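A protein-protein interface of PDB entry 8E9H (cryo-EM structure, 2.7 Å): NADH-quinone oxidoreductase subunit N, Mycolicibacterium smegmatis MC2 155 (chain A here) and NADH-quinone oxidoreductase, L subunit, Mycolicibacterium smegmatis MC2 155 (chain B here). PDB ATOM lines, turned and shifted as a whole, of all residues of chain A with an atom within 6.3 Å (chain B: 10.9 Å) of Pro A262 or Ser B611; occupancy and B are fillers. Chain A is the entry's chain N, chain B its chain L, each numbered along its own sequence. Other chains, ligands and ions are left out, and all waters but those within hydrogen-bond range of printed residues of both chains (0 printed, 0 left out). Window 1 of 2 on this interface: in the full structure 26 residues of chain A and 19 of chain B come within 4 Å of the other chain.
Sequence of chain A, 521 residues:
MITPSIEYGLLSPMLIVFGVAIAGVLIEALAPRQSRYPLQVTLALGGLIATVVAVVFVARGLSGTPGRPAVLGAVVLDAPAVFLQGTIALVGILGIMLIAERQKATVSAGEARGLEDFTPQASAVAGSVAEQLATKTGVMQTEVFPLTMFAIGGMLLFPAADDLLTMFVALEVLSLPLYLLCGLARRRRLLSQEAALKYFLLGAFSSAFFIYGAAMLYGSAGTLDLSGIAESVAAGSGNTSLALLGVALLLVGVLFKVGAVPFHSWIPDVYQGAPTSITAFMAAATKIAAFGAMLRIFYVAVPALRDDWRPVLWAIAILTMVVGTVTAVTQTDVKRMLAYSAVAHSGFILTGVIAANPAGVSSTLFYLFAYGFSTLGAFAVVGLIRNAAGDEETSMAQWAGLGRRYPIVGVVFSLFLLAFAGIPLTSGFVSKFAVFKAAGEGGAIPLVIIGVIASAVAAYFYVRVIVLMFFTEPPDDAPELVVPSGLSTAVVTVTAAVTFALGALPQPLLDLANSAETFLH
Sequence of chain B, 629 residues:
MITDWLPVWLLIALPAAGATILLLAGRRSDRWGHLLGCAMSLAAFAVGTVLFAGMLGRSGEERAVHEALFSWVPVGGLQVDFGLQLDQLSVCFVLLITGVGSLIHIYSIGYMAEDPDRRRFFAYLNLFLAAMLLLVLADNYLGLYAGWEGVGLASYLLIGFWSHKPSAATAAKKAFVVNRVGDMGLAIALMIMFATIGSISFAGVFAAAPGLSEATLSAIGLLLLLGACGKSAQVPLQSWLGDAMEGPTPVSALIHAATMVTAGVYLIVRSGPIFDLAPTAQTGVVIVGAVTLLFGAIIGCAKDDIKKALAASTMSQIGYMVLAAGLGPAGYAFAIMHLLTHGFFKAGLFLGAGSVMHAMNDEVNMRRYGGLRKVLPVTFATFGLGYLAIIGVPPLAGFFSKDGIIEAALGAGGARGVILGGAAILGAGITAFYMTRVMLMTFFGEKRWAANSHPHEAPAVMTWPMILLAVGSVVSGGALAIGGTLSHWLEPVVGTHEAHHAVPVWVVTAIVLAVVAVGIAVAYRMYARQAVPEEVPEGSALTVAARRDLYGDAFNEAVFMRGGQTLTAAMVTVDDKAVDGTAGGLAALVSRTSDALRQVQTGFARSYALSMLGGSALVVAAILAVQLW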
ATOM      1  N   PHE A 205       3.624  18.400  14.876  1.00  0.00           N
ATOM      2  CA  PHE A 205       4.885  17.690  14.712  1.00  0.00           C
ATOM      3  C   PHE A 205       6.000  18.426  15.462  1.00  0.00           C
ATOM      4  O   PHE A 205       6.737  17.839  16.273  1.00  0.00           O
ATOM      5  CB  PHE A 205       5.125  17.585  13.201  1.00  0.00           C
ATOM      6  CG  PHE A 205       6.344  16.830  12.781  1.00  0.00           C
ATOM      7  CD1 PHE A 205       6.367  15.448  12.834  1.00  0.00           C
ATOM      8  CD2 PHE A 205       7.423  17.489  12.225  1.00  0.00           C
ATOM      9  CE1 PHE A 205       7.470  14.747  12.404  1.00  0.00           C
ATOM     10  CE2 PHE A 205       8.522  16.788  11.787  1.00  0.00           C
ATOM     11  CZ  PHE A 205       8.545  15.416  11.878  1.00  0.00           C
ATOM     12  N   LEU A 255      12.256  27.035  16.409  1.00  0.00           N
ATOM     13  CA  LEU A 255      12.617  27.418  15.051  1.00  0.00           C
ATOM     14  C   LEU A 255      11.444  27.238  14.105  1.00  0.00           C
ATOM     15  O   LEU A 255      11.214  28.072  13.223  1.00  0.00           O
ATOM     16  CB  LEU A 255      13.808  26.597  14.569  1.00  0.00           C
ATOM     17  CG  LEU A 255      15.167  26.918  15.185  1.00  0.00           C
ATOM     18  CD1 LEU A 255      16.197  25.945  14.656  1.00  0.00           C
ATOM     19  CD2 LEU A 255      15.589  28.342  14.899  1.00  0.00           C
ATOM     20  N   GLY A 259      10.300  30.014  11.966  1.00  0.00           N
ATOM     21  CA  GLY A 259      10.397  29.768  10.540  1.00  0.00           C
ATOM     22  C   GLY A 259      11.797  29.684   9.972  1.00  0.00           C
ATOM     23  O   GLY A 259      12.074  30.296   8.936  1.00  0.00           O
ATOM     24  N   ALA A 260      12.691  28.939  10.614  1.00  0.00           N
ATOM     25  CA  ALA A 260      13.990  28.669  10.022  1.00  0.00           C
ATOM     26  C   ALA A 260      13.834  27.752   8.810  1.00  0.00           C
ATOM     27  O   ALA A 260      12.871  26.989   8.700  1.00  0.00           O
ATOM     28  CB  ALA A 260      14.921  28.035  11.048  1.00  0.00           C
ATOM     29  N   VAL A 261      14.803  27.826   7.891  1.00  0.00           N
ATOM     30  CA  VAL A 261      14.663  27.120   6.615  1.00  0.00           C
ATOM     31  C   VAL A 261      14.376  25.637   6.790  1.00  0.00           C
ATOM     32  O   VAL A 261      13.460  25.126   6.126  1.00  0.00           O
ATOM     33  CB  VAL A 261      15.892  27.375   5.725  1.00  0.00           C
ATOM     34  CG1 VAL A 261      15.806  26.544   4.464  1.00  0.00           C
ATOM     35  CG2 VAL A 261      15.890  28.801   5.316  1.00  0.00           C
ATOM     36  N   PRO A 262      15.090  24.895   7.634  1.00  0.00           N
ATOM     37  CA  PRO A 262      14.726  23.487   7.820  1.00  0.00           C
ATOM     38  C   PRO A 262      13.292  23.320   8.271  1.00  0.00           C
ATOM     39  O   PRO A 262      12.744  22.218   8.161  1.00  0.00           O
ATOM     40  CB  PRO A 262      15.717  23.003   8.886  1.00  0.00           C
ATOM     41  CG  PRO A 262      16.860  23.951   8.803  1.00  0.00           C
ATOM     42  CD  PRO A 262      16.271  25.273   8.424  1.00  0.00           C
ATOM     43  N   PHE A 263      12.659  24.387   8.761  1.00  0.00           N
ATOM     44  CA  PHE A 263      11.301  24.336   9.275  1.00  0.00           C
ATOM     45  C   PHE A 263      10.426  25.433   8.687  1.00  0.00           C
ATOM     46  O   PHE A 263       9.333  25.685   9.199  1.00  0.00           O
ATOM     47  CB  PHE A 263      11.341  24.449  10.797  1.00  0.00           C
ATOM     48  CG  PHE A 263      12.302  23.496  11.433  1.00  0.00           C
ATOM     49  CD1 PHE A 263      11.919  22.210  11.750  1.00  0.00           C
ATOM     50  CD2 PHE A 263      13.597  23.891  11.709  1.00  0.00           C
ATOM     51  CE1 PHE A 263      12.812  21.336  12.326  1.00  0.00           C
ATOM     52  CE2 PHE A 263      14.491  23.022  12.288  1.00  0.00           C
ATOM     53  CZ  PHE A 263      14.098  21.745  12.596  1.00  0.00           C
ATOM     54  N   HIS A 264      10.885  26.093   7.624  1.00  0.00           N
ATOM     55  CA  HIS A 264      10.188  27.264   7.106  1.00  0.00           C
ATOM     56  C   HIS A 264       8.971  26.885   6.277  1.00  0.00           C
ATOM     57  O   HIS A 264       7.987  27.628   6.251  1.00  0.00           O
ATOM     58  CB  HIS A 264      11.141  28.082   6.244  1.00  0.00           C
ATOM     59  CG  HIS A 264      11.355  27.504   4.881  1.00  0.00           C
ATOM     60  ND1 HIS A 264      12.423  26.691   4.572  1.00  0.00           N
ATOM     61  CD2 HIS A 264      10.646  27.642   3.735  1.00  0.00           C
ATOM     62  CE1 HIS A 264      12.352  26.335   3.302  1.00  0.00           C
ATOM     63  NE2 HIS A 264      11.285  26.901   2.771  1.00  0.00           N
ATOM     64  N   SER A 265       9.025  25.738   5.597  1.00  0.00           N
ATOM     65  CA  SER A 265       8.117  25.468   4.490  1.00  0.00           C
ATOM     66  C   SER A 265       6.664  25.753   4.827  1.00  0.00           C
ATOM     67  O   SER A 265       5.867  25.999   3.916  1.00  0.00           O
ATOM     68  CB  SER A 265       8.265  24.016   4.050  1.00  0.00           C
ATOM     69  OG  SER A 265       9.502  23.812   3.393  1.00  0.00           O
ATOM     70  N   ILE A 316      21.879  27.390  10.751  1.00  0.00           N
ATOM     71  CA  ILE A 316      20.489  27.749  10.507  1.00  0.00           C
ATOM     72  C   ILE A 316      20.397  29.195  10.049  1.00  0.00           C
ATOM     73  O   ILE A 316      19.824  29.493   8.994  1.00  0.00           O
ATOM     74  CB  ILE A 316      19.640  27.501  11.762  1.00  0.00           C
ATOM     75  CG1 ILE A 316      19.526  26.005  12.035  1.00  0.00           C
ATOM     76  CG2 ILE A 316      18.265  28.094  11.587  1.00  0.00           C
ATOM     77  CD1 ILE A 316      19.512  25.670  13.493  1.00  0.00           C
ATOM     78  N   LEU A 319      21.433  29.700   6.545  1.00  0.00           N
ATOM     79  CA  LEU A 319      20.376  29.155   5.704  1.00  0.00           C
ATOM     80  C   LEU A 319      19.164  30.068   5.699  1.00  0.00           C
ATOM     81  O   LEU A 319      18.662  30.441   4.632  1.00  0.00           O
ATOM     82  CB  LEU A 319      19.977  27.766   6.193  1.00  0.00           C
ATOM     83  CG  LEU A 319      20.941  26.627   5.881  1.00  0.00           C
ATOM     84  CD1 LEU A 319      20.573  25.407   6.699  1.00  0.00           C
ATOM     85  CD2 LEU A 319      20.916  26.308   4.401  1.00  0.00           C
ATOM     86  N   THR A 320      18.696  30.462   6.882  1.00  0.00           N
ATOM     87  CA  THR A 320      17.483  31.263   6.962  1.00  0.00           C
ATOM     88  C   THR A 320      17.641  32.565   6.198  1.00  0.00           C
ATOM     89  O   THR A 320      16.684  33.055   5.590  1.00  0.00           O
ATOM     90  CB  THR A 320      17.128  31.526   8.419  1.00  0.00           C
ATOM     91  OG1 THR A 320      17.145  30.292   9.140  1.00  0.00           O
ATOM     92  CG2 THR A 320      15.746  32.118   8.509  1.00  0.00           C
ATOM     93  N   LEU B 597      15.158  26.195  -5.439  1.00  0.00           N
ATOM     94  CA  LEU B 597      14.661  26.182  -4.069  1.00  0.00           C
ATOM     95  C   LEU B 597      13.141  26.185  -4.034  1.00  0.00           C
ATOM     96  O   LEU B 597      12.531  25.472  -3.232  1.00  0.00           O
ATOM     97  CB  LEU B 597      15.209  27.382  -3.301  1.00  0.00           C
ATOM     98  CG  LEU B 597      16.705  27.361  -2.997  1.00  0.00           C
ATOM     99  CD1 LEU B 597      17.141  28.703  -2.448  1.00  0.00           C
ATOM    100  CD2 LEU B 597      17.038  26.255  -2.018  1.00  0.00           C
ATOM    101  N   ARG B 598      12.510  26.983  -4.894  1.00  0.00           N
ATOM    102  CA  ARG B 598      11.055  27.009  -4.935  1.00  0.00           C
ATOM    103  C   ARG B 598      10.496  25.653  -5.327  1.00  0.00           C
ATOM    104  O   ARG B 598       9.402  25.282  -4.889  1.00  0.00           O
ATOM    105  CB  ARG B 598      10.585  28.085  -5.907  1.00  0.00           C
ATOM    106  CG  ARG B 598       9.091  28.290  -5.912  1.00  0.00           C
ATOM    107  CD  ARG B 598       8.724  29.567  -6.630  1.00  0.00           C
ATOM    108  NE  ARG B 598       9.179  29.548  -8.014  1.00  0.00           N
ATOM    109  CZ  ARG B 598       8.557  30.146  -9.020  1.00  0.00           C
ATOM    110  NH1 ARG B 598       7.438  30.829  -8.837  1.00  0.00           N
ATOM    111  NH2 ARG B 598       9.072  30.060 -10.243  1.00  0.00           N
ATOM    112  N   GLN B 599      11.228  24.898  -6.145  1.00  0.00           N
ATOM    113  CA  GLN B 599      10.818  23.532  -6.435  1.00  0.00           C
ATOM    114  C   GLN B 599      10.766  22.673  -5.178  1.00  0.00           C
ATOM    115  O   GLN B 599      10.050  21.667  -5.159  1.00  0.00           O
ATOM    116  CB  GLN B 599      11.765  22.902  -7.455  1.00  0.00           C
ATOM    117  N   VAL B 600      11.507  23.043  -4.130  1.00  0.00           N
ATOM    118  CA  VAL B 600      11.444  22.297  -2.877  1.00  0.00           C
ATOM    119  C   VAL B 600      10.096  22.490  -2.199  1.00  0.00           C
ATOM    120  O   VAL B 600       9.633  21.612  -1.463  1.00  0.00           O
ATOM    121  CB  VAL B 600      12.595  22.714  -1.946  1.00  0.00           C
ATOM    122  CG1 VAL B 600      12.525  21.947  -0.641  1.00  0.00           C
ATOM    123  CG2 VAL B 600      13.932  22.487  -2.626  1.00  0.00           C
ATOM    124  N   GLN B 601       9.454  23.636  -2.411  1.00  0.00           N
ATOM    125  CA  GLN B 601       8.139  23.910  -1.835  1.00  0.00           C
ATOM    126  C   GLN B 601       7.066  23.121  -2.587  1.00  0.00           C
ATOM    127  O   GLN B 601       6.194  23.669  -3.259  1.00  0.00           O
ATOM    128  CB  GLN B 601       7.859  25.405  -1.872  1.00  0.00           C
ATOM    129  CG  GLN B 601       6.685  25.841  -1.027  1.00  0.00           C
ATOM    130  CD  GLN B 601       6.999  25.836   0.449  1.00  0.00           C
ATOM    131  OE1 GLN B 601       8.145  25.641   0.851  1.00  0.00           O
ATOM    132  NE2 GLN B 601       5.979  26.051   1.269  1.00  0.00           N
ATOM    133  N   THR B 602       7.140  21.797  -2.449  1.00  0.00           N
ATOM    134  CA  THR B 602       6.286  20.918  -3.238  1.00  0.00           C
ATOM    135  C   THR B 602       4.809  21.129  -2.951  1.00  0.00           C
ATOM    136  O   THR B 602       3.974  20.795  -3.796  1.00  0.00           O
ATOM    137  CB  THR B 602       6.644  19.454  -2.983  1.00  0.00           C
ATOM    138  OG1 THR B 602       6.190  19.070  -1.681  1.00  0.00           O
ATOM    139  CG2 THR B 602       8.143  19.237  -3.083  1.00  0.00           C
ATOM    140  N   GLY B 603       4.465  21.671  -1.788  1.00  0.00           N
ATOM    141  CA  GLY B 603       3.085  21.844  -1.402  1.00  0.00           C
ATOM    142  C   GLY B 603       2.494  20.681  -0.638  1.00  0.00           C
ATOM    143  O   GLY B 603       1.355  20.781  -0.175  1.00  0.00           O
ATOM    144  N   PHE B 604       3.227  19.583  -0.497  1.00  0.00           N
ATOM    145  CA  PHE B 604       2.748  18.441   0.267  1.00  0.00           C
ATOM    146  C   PHE B 604       3.162  18.599   1.721  1.00  0.00           C
ATOM    147  O   PHE B 604       4.345  18.791   2.017  1.00  0.00           O
ATOM    148  CB  PHE B 604       3.303  17.144  -0.309  1.00  0.00           C
ATOM    149  CG  PHE B 604       2.782  16.820  -1.671  1.00  0.00           C
ATOM    150  CD1 PHE B 604       1.490  16.371  -1.840  1.00  0.00           C
ATOM    151  CD2 PHE B 604       3.585  16.964  -2.784  1.00  0.00           C
ATOM    152  CE1 PHE B 604       1.006  16.072  -3.090  1.00  0.00           C
ATOM    153  CE2 PHE B 604       3.106  16.668  -4.038  1.00  0.00           C
ATOM    154  CZ  PHE B 604       1.815  16.220  -4.192  1.00  0.00           C
ATOM    155  N   ALA B 605       2.192  18.507   2.629  1.00  0.00           N
ATOM    156  CA  ALA B 605       2.505  18.624   4.047  1.00  0.00           C
ATOM    157  C   ALA B 605       3.525  17.579   4.468  1.00  0.00           C
ATOM    158  O   ALA B 605       4.359  17.830   5.342  1.00  0.00           O
ATOM    159  CB  ALA B 605       1.230  18.491   4.876  1.00  0.00           C
ATOM    160  N   ARG B 606       3.476  16.397   3.854  1.00  0.00           N
ATOM    161  CA  ARG B 606       4.395  15.335   4.242  1.00  0.00           C
ATOM    162  C   ARG B 606       5.825  15.653   3.832  1.00  0.00           C
ATOM    163  O   ARG B 606       6.766  15.310   4.555  1.00  0.00           O
ATOM    164  CB  ARG B 606       3.937  14.009   3.643  1.00  0.00           C
ATOM    165  CG  ARG B 606       2.660  13.502   4.274  1.00  0.00           C
ATOM    166  CD  ARG B 606       2.322  12.086   3.868  1.00  0.00           C
ATOM    167  NE  ARG B 606       2.273  11.919   2.421  1.00  0.00           N
ATOM    168  CZ  ARG B 606       2.929  10.989   1.740  1.00  0.00           C
ATOM    169  NH1 ARG B 606       3.700  10.098   2.343  1.00  0.00           N
ATOM    170  NH2 ARG B 606       2.805  10.946   0.418  1.00  0.00           N
ATOM    171  N   SER B 607       6.019  16.307   2.689  1.00  0.00           N
ATOM    172  CA  SER B 607       7.363  16.735   2.321  1.00  0.00           C
ATOM    173  C   SER B 607       7.904  17.764   3.303  1.00  0.00           C
ATOM    174  O   SER B 607       9.082  17.710   3.679  1.00  0.00           O
ATOM    175  CB  SER B 607       7.360  17.298   0.905  1.00  0.00           C
ATOM    176  OG  SER B 607       6.757  18.577   0.878  1.00  0.00           O
ATOM    177  N   TYR B 608       7.065  18.705   3.733  1.00  0.00           N
ATOM    178  CA  TYR B 608       7.498  19.662   4.743  1.00  0.00           C
ATOM    179  C   TYR B 608       7.833  18.958   6.047  1.00  0.00           C
ATOM    180  O   TYR B 608       8.792  19.327   6.731  1.00  0.00           O
ATOM    181  CB  TYR B 608       6.412  20.707   4.978  1.00  0.00           C
ATOM    182  CG  TYR B 608       5.994  21.466   3.744  1.00  0.00           C
ATOM    183  CD1 TYR B 608       6.743  21.414   2.579  1.00  0.00           C
ATOM    184  CD2 TYR B 608       4.847  22.237   3.748  1.00  0.00           C
ATOM    185  CE1 TYR B 608       6.360  22.110   1.460  1.00  0.00           C
ATOM    186  CE2 TYR B 608       4.456  22.930   2.636  1.00  0.00           C
ATOM    187  CZ  TYR B 608       5.215  22.866   1.494  1.00  0.00           C
ATOM    188  OH  TYR B 608       4.825  23.566   0.379  1.00  0.00           O
ATOM    189  N   ALA B 609       7.041  17.953   6.416  1.00  0.00           N
ATOM    190  CA  ALA B 609       7.340  17.189   7.619  1.00  0.00           C
ATOM    191  C   ALA B 609       8.676  16.475   7.486  1.00  0.00           C
ATOM    192  O   ALA B 609       9.436  16.379   8.454  1.00  0.00           O
ATOM    193  CB  ALA B 609       6.219  16.192   7.897  1.00  0.00           C
ATOM    194  N   LEU B 610       8.972  15.954   6.297  1.00  0.00           N
ATOM    195  CA  LEU B 610      10.275  15.342   6.069  1.00  0.00           C
ATOM    196  C   LEU B 610      11.391  16.360   6.251  1.00  0.00           C
ATOM    197  O   LEU B 610      12.407  16.081   6.898  1.00  0.00           O
ATOM    198  CB  LEU B 610      10.326  14.736   4.669  1.00  0.00           C
ATOM    199  CG  LEU B 610      11.704  14.339   4.151  1.00  0.00           C
ATOM    200  CD1 LEU B 610      12.286  13.244   5.015  1.00  0.00           C
ATOM    201  CD2 LEU B 610      11.610  13.890   2.709  1.00  0.00           C
ATOM    202  N   SER B 611      11.216  17.558   5.695  1.00  0.00           N
ATOM    203  CA  SER B 611      12.230  18.589   5.873  1.00  0.00           C
ATOM    204  C   SER B 611      12.425  18.906   7.348  1.00  0.00           C
ATOM    205  O   SER B 611      13.560  19.025   7.823  1.00  0.00           O
ATOM    206  CB  SER B 611      11.844  19.850   5.103  1.00  0.00           C
ATOM    207  OG  SER B 611      11.633  19.564   3.733  1.00  0.00           O
ATOM    208  N   MET B 612      11.327  19.033   8.092  1.00  0.00           N
ATOM    209  CA  MET B 612      11.426  19.294   9.523  1.00  0.00           C
ATOM    210  C   MET B 612      12.155  18.174  10.250  1.00  0.00           C
ATOM    211  O   MET B 612      13.036  18.443  11.071  1.00  0.00           O
ATOM    212  CB  MET B 612      10.036  19.475  10.120  1.00  0.00           C
ATOM    213  CG  MET B 612       9.317  20.708   9.638  1.00  0.00           C
ATOM    214  SD  MET B 612       7.661  20.792  10.322  1.00  0.00           S
ATOM    215  CE  MET B 612       8.046  21.145  12.030  1.00  0.00           C
ATOM    216  N   LEU B 613      11.814  16.922   9.957  1.00  0.00           N
ATOM    217  CA  LEU B 613      12.537  15.794  10.521  1.00  0.00           C
ATOM    218  C   LEU B 613      13.997  15.805  10.110  1.00  0.00           C
ATOM    219  O   LEU B 613      14.814  15.129  10.741  1.00  0.00           O
ATOM    220  CB  LEU B 613      11.889  14.479  10.092  1.00  0.00           C
ATOM    221  CG  LEU B 613      12.329  13.247  10.880  1.00  0.00           C
ATOM    222  CD1 LEU B 613      11.923  13.367  12.329  1.00  0.00           C
ATOM    223  CD2 LEU B 613      11.743  11.996  10.273  1.00  0.00           C
ATOM    224  N   GLY B 614      14.329  16.550   9.062  1.00  0.00           N
ATOM    225  CA  GLY B 614      15.702  16.931   8.802  1.00  0.00           C
ATOM    226  C   GLY B 614      16.343  17.617   9.996  1.00  0.00           C
ATOM    227  O   GLY B 614      17.559  17.830  10.012  1.00  0.00           O
ATOM    228  N   GLY B 615      15.540  17.977  11.004  1.00  0.00           N
ATOM    229  CA  GLY B 615      16.080  18.412  12.282  1.00  0.00           C
ATOM    230  C   GLY B 615      17.013  17.403  12.919  1.00  0.00           C
ATOM    231  O   GLY B 615      17.703  17.726  13.894  1.00  0.00           O
ATOM    232  N   SER B 616      17.046  16.176  12.398  1.00  0.00           N
ATOM    233  CA  SER B 616      18.141  15.281  12.737  1.00  0.00           C
ATOM    234  C   SER B 616      19.473  15.924  12.399  1.00  0.00           C
ATOM    235  O   SER B 616      20.483  15.648  13.055  1.00  0.00           O
ATOM    236  CB  SER B 616      17.987  13.957  11.993  1.00  0.00           C
ATOM    237  OG  SER B 616      17.889  14.176  10.598  1.00  0.00           O
ATOM    238  N   ALA B 617      19.497  16.787  11.382  1.00  0.00           N
ATOM    239  CA  ALA B 617      20.703  17.553  11.100  1.00  0.00           C
ATOM    240  C   ALA B 617      21.064  18.447  12.277  1.00  0.00           C
ATOM    241  O   ALA B 617      22.231  18.521  12.673  1.00  0.00           O
ATOM    242  CB  ALA B 617      20.514  18.384   9.832  1.00  0.00           C
ATOM    243  N   LEU B 618      20.075  19.123  12.862  1.00  0.00           N
ATOM    244  CA  LEU B 618      20.335  19.933  14.047  1.00  0.00           C
ATOM    245  C   LEU B 618      20.861  19.074  15.183  1.00  0.00           C
ATOM    246  O   LEU B 618      21.806  19.451  15.884  1.00  0.00           O
ATOM    247  CB  LEU B 618      19.062  20.649  14.487  1.00  0.00           C
ATOM    248  CG  LEU B 618      18.793  21.999  13.840  1.00  0.00           C
ATOM    249  CD1 LEU B 618      18.716  21.861  12.332  1.00  0.00           C
ATOM    250  CD2 LEU B 618      17.509  22.583  14.396  1.00  0.00           C
ATOM    251  N   VAL B 619      20.239  17.916  15.392  1.00  0.00           N
ATOM    252  CA  VAL B 619      20.640  17.053  16.500  1.00  0.00           C
ATOM    253  C   VAL B 619      22.085  16.603  16.324  1.00  0.00           C
ATOM    254  O   VAL B 619      22.899  16.678  17.254  1.00  0.00           O
ATOM    255  CB  VAL B 619      19.687  15.852  16.616  1.00  0.00           C
ATOM    256  CG1 VAL B 619      20.175  14.896  17.685  1.00  0.00           C
ATOM    257  CG2 VAL B 619      18.286  16.328  16.930  1.00  0.00           C
ATOM    258  N   ALA B 621      24.391  17.978  14.504  1.00  0.00           N
ATOM    259  CA  ALA B 621      25.295  19.117  14.598  1.00  0.00           C
ATOM    260  C   ALA B 621      25.576  19.470  16.049  1.00  0.00           C
ATOM    261  O   ALA B 621      26.728  19.710  16.427  1.00  0.00           O
ATOM    262  CB  ALA B 621      24.706  20.315  13.859  1.00  0.00           C
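The side-chain amide nitrogen of Gln B601 lies within hydrogen-bond range of the backbone carbonyl oxygen of Ser A265, at 2.6 Å.
O of Pro A262 sits close to N of Met B612 (3.5 Å).
The backbone carbonyl oxygen (O) of Pro A262 lies close to the backbone carbonyl oxygen (O) of Ser B611 (3.3 Å).
NE2 of Gln B601 lies within hydrogen-bond range of OH of Tyr B608 (2.9 Å).
The backbone carbonyl oxygen (O) of Ser B607 sits at hydrogen-bond distance from the side-chain hydroxyl (OG) of Ser B611.
O of Leu B613 lies within hydrogen-bond range of OG of Ser B616.
O of Leu A255 is in hydrogen-bond range of N of Ala A260, 3.1 Å away.
A ring nitrogen (ND1) of His A264 sits at hydrogen-bond distance from the backbone carbonyl oxygen (O) of Val A261 (2.4 Å).
The backbone carbonyl oxygen of Ile A316 lies within hydrogen-bond range of the side-chain hydroxyl of Thr A320 (2.8 Å).
Among the printed residues, merely in contact across the chains: Phe A205 with Ala B609, Phe A205 with Met B612, Phe A205 with Leu B613, Leu A255 with Leu B618, Phe A263 with Met B612, Phe A263 with Gly B615, Phe A263 with Leu B618, His A264 with Gln B601, Ser A265 with Tyr B608 and Ile A316 with Leu B618.
Pro A262 touches two residues of chain B.
Of chain A, only Pro A262 (3.3 Å) comes within 4 Å of Ser B611.
No residue of chain B comes within 4 Å of Ala A260.
No residue of chain B comes within 4 Å of Val A261.
Of chain B, only Leu B618 comes within 4 Å of Ile A316.
Printed residues of chain B within 4 Å of Phe A205: Ala B609, Met B612 and Leu B613.
Printed residues of chain A within 4 Å of Met B612: Phe A205, Pro A262 and Phe A263.
Printed residues of chain A within 4 Å of Gly B615: Phe A263.
Printed residues of chain B within 4 Å of Ser A265: Gln B601 (2.6 Å) and Tyr B608 (3.4 Å).
Of the printed residues of chain A, Leu B613 touches Phe A205.
Gln B599 touches none of the printed residues of chain A.
Val B619 touches none of the printed residues of chain A.
The nearest residue of chain B that does not touch Pro A262 is Leu B618 (4.5 Å).
The nearest residue of chain A that does not touch Ser B611 is Ser A265 (4.8 Å).
The nearest printed residue of chain A that does not touch Leu B618 is Pro A262 (4.5 Å).
Along chain B the printed residues that touch a printed residue of chain A span positions 601 to 618.
Of the 12 printed residues of chain A, 7 touch a printed residue of chain B.
Hydrophobic or aromatic side chains of chain A within 4 Å of the printed part of chain B: Phe A205, Leu A255, Phe A263, His A264 and Ile A316.
Among the printed residues, 13 pairs touch across the chains.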
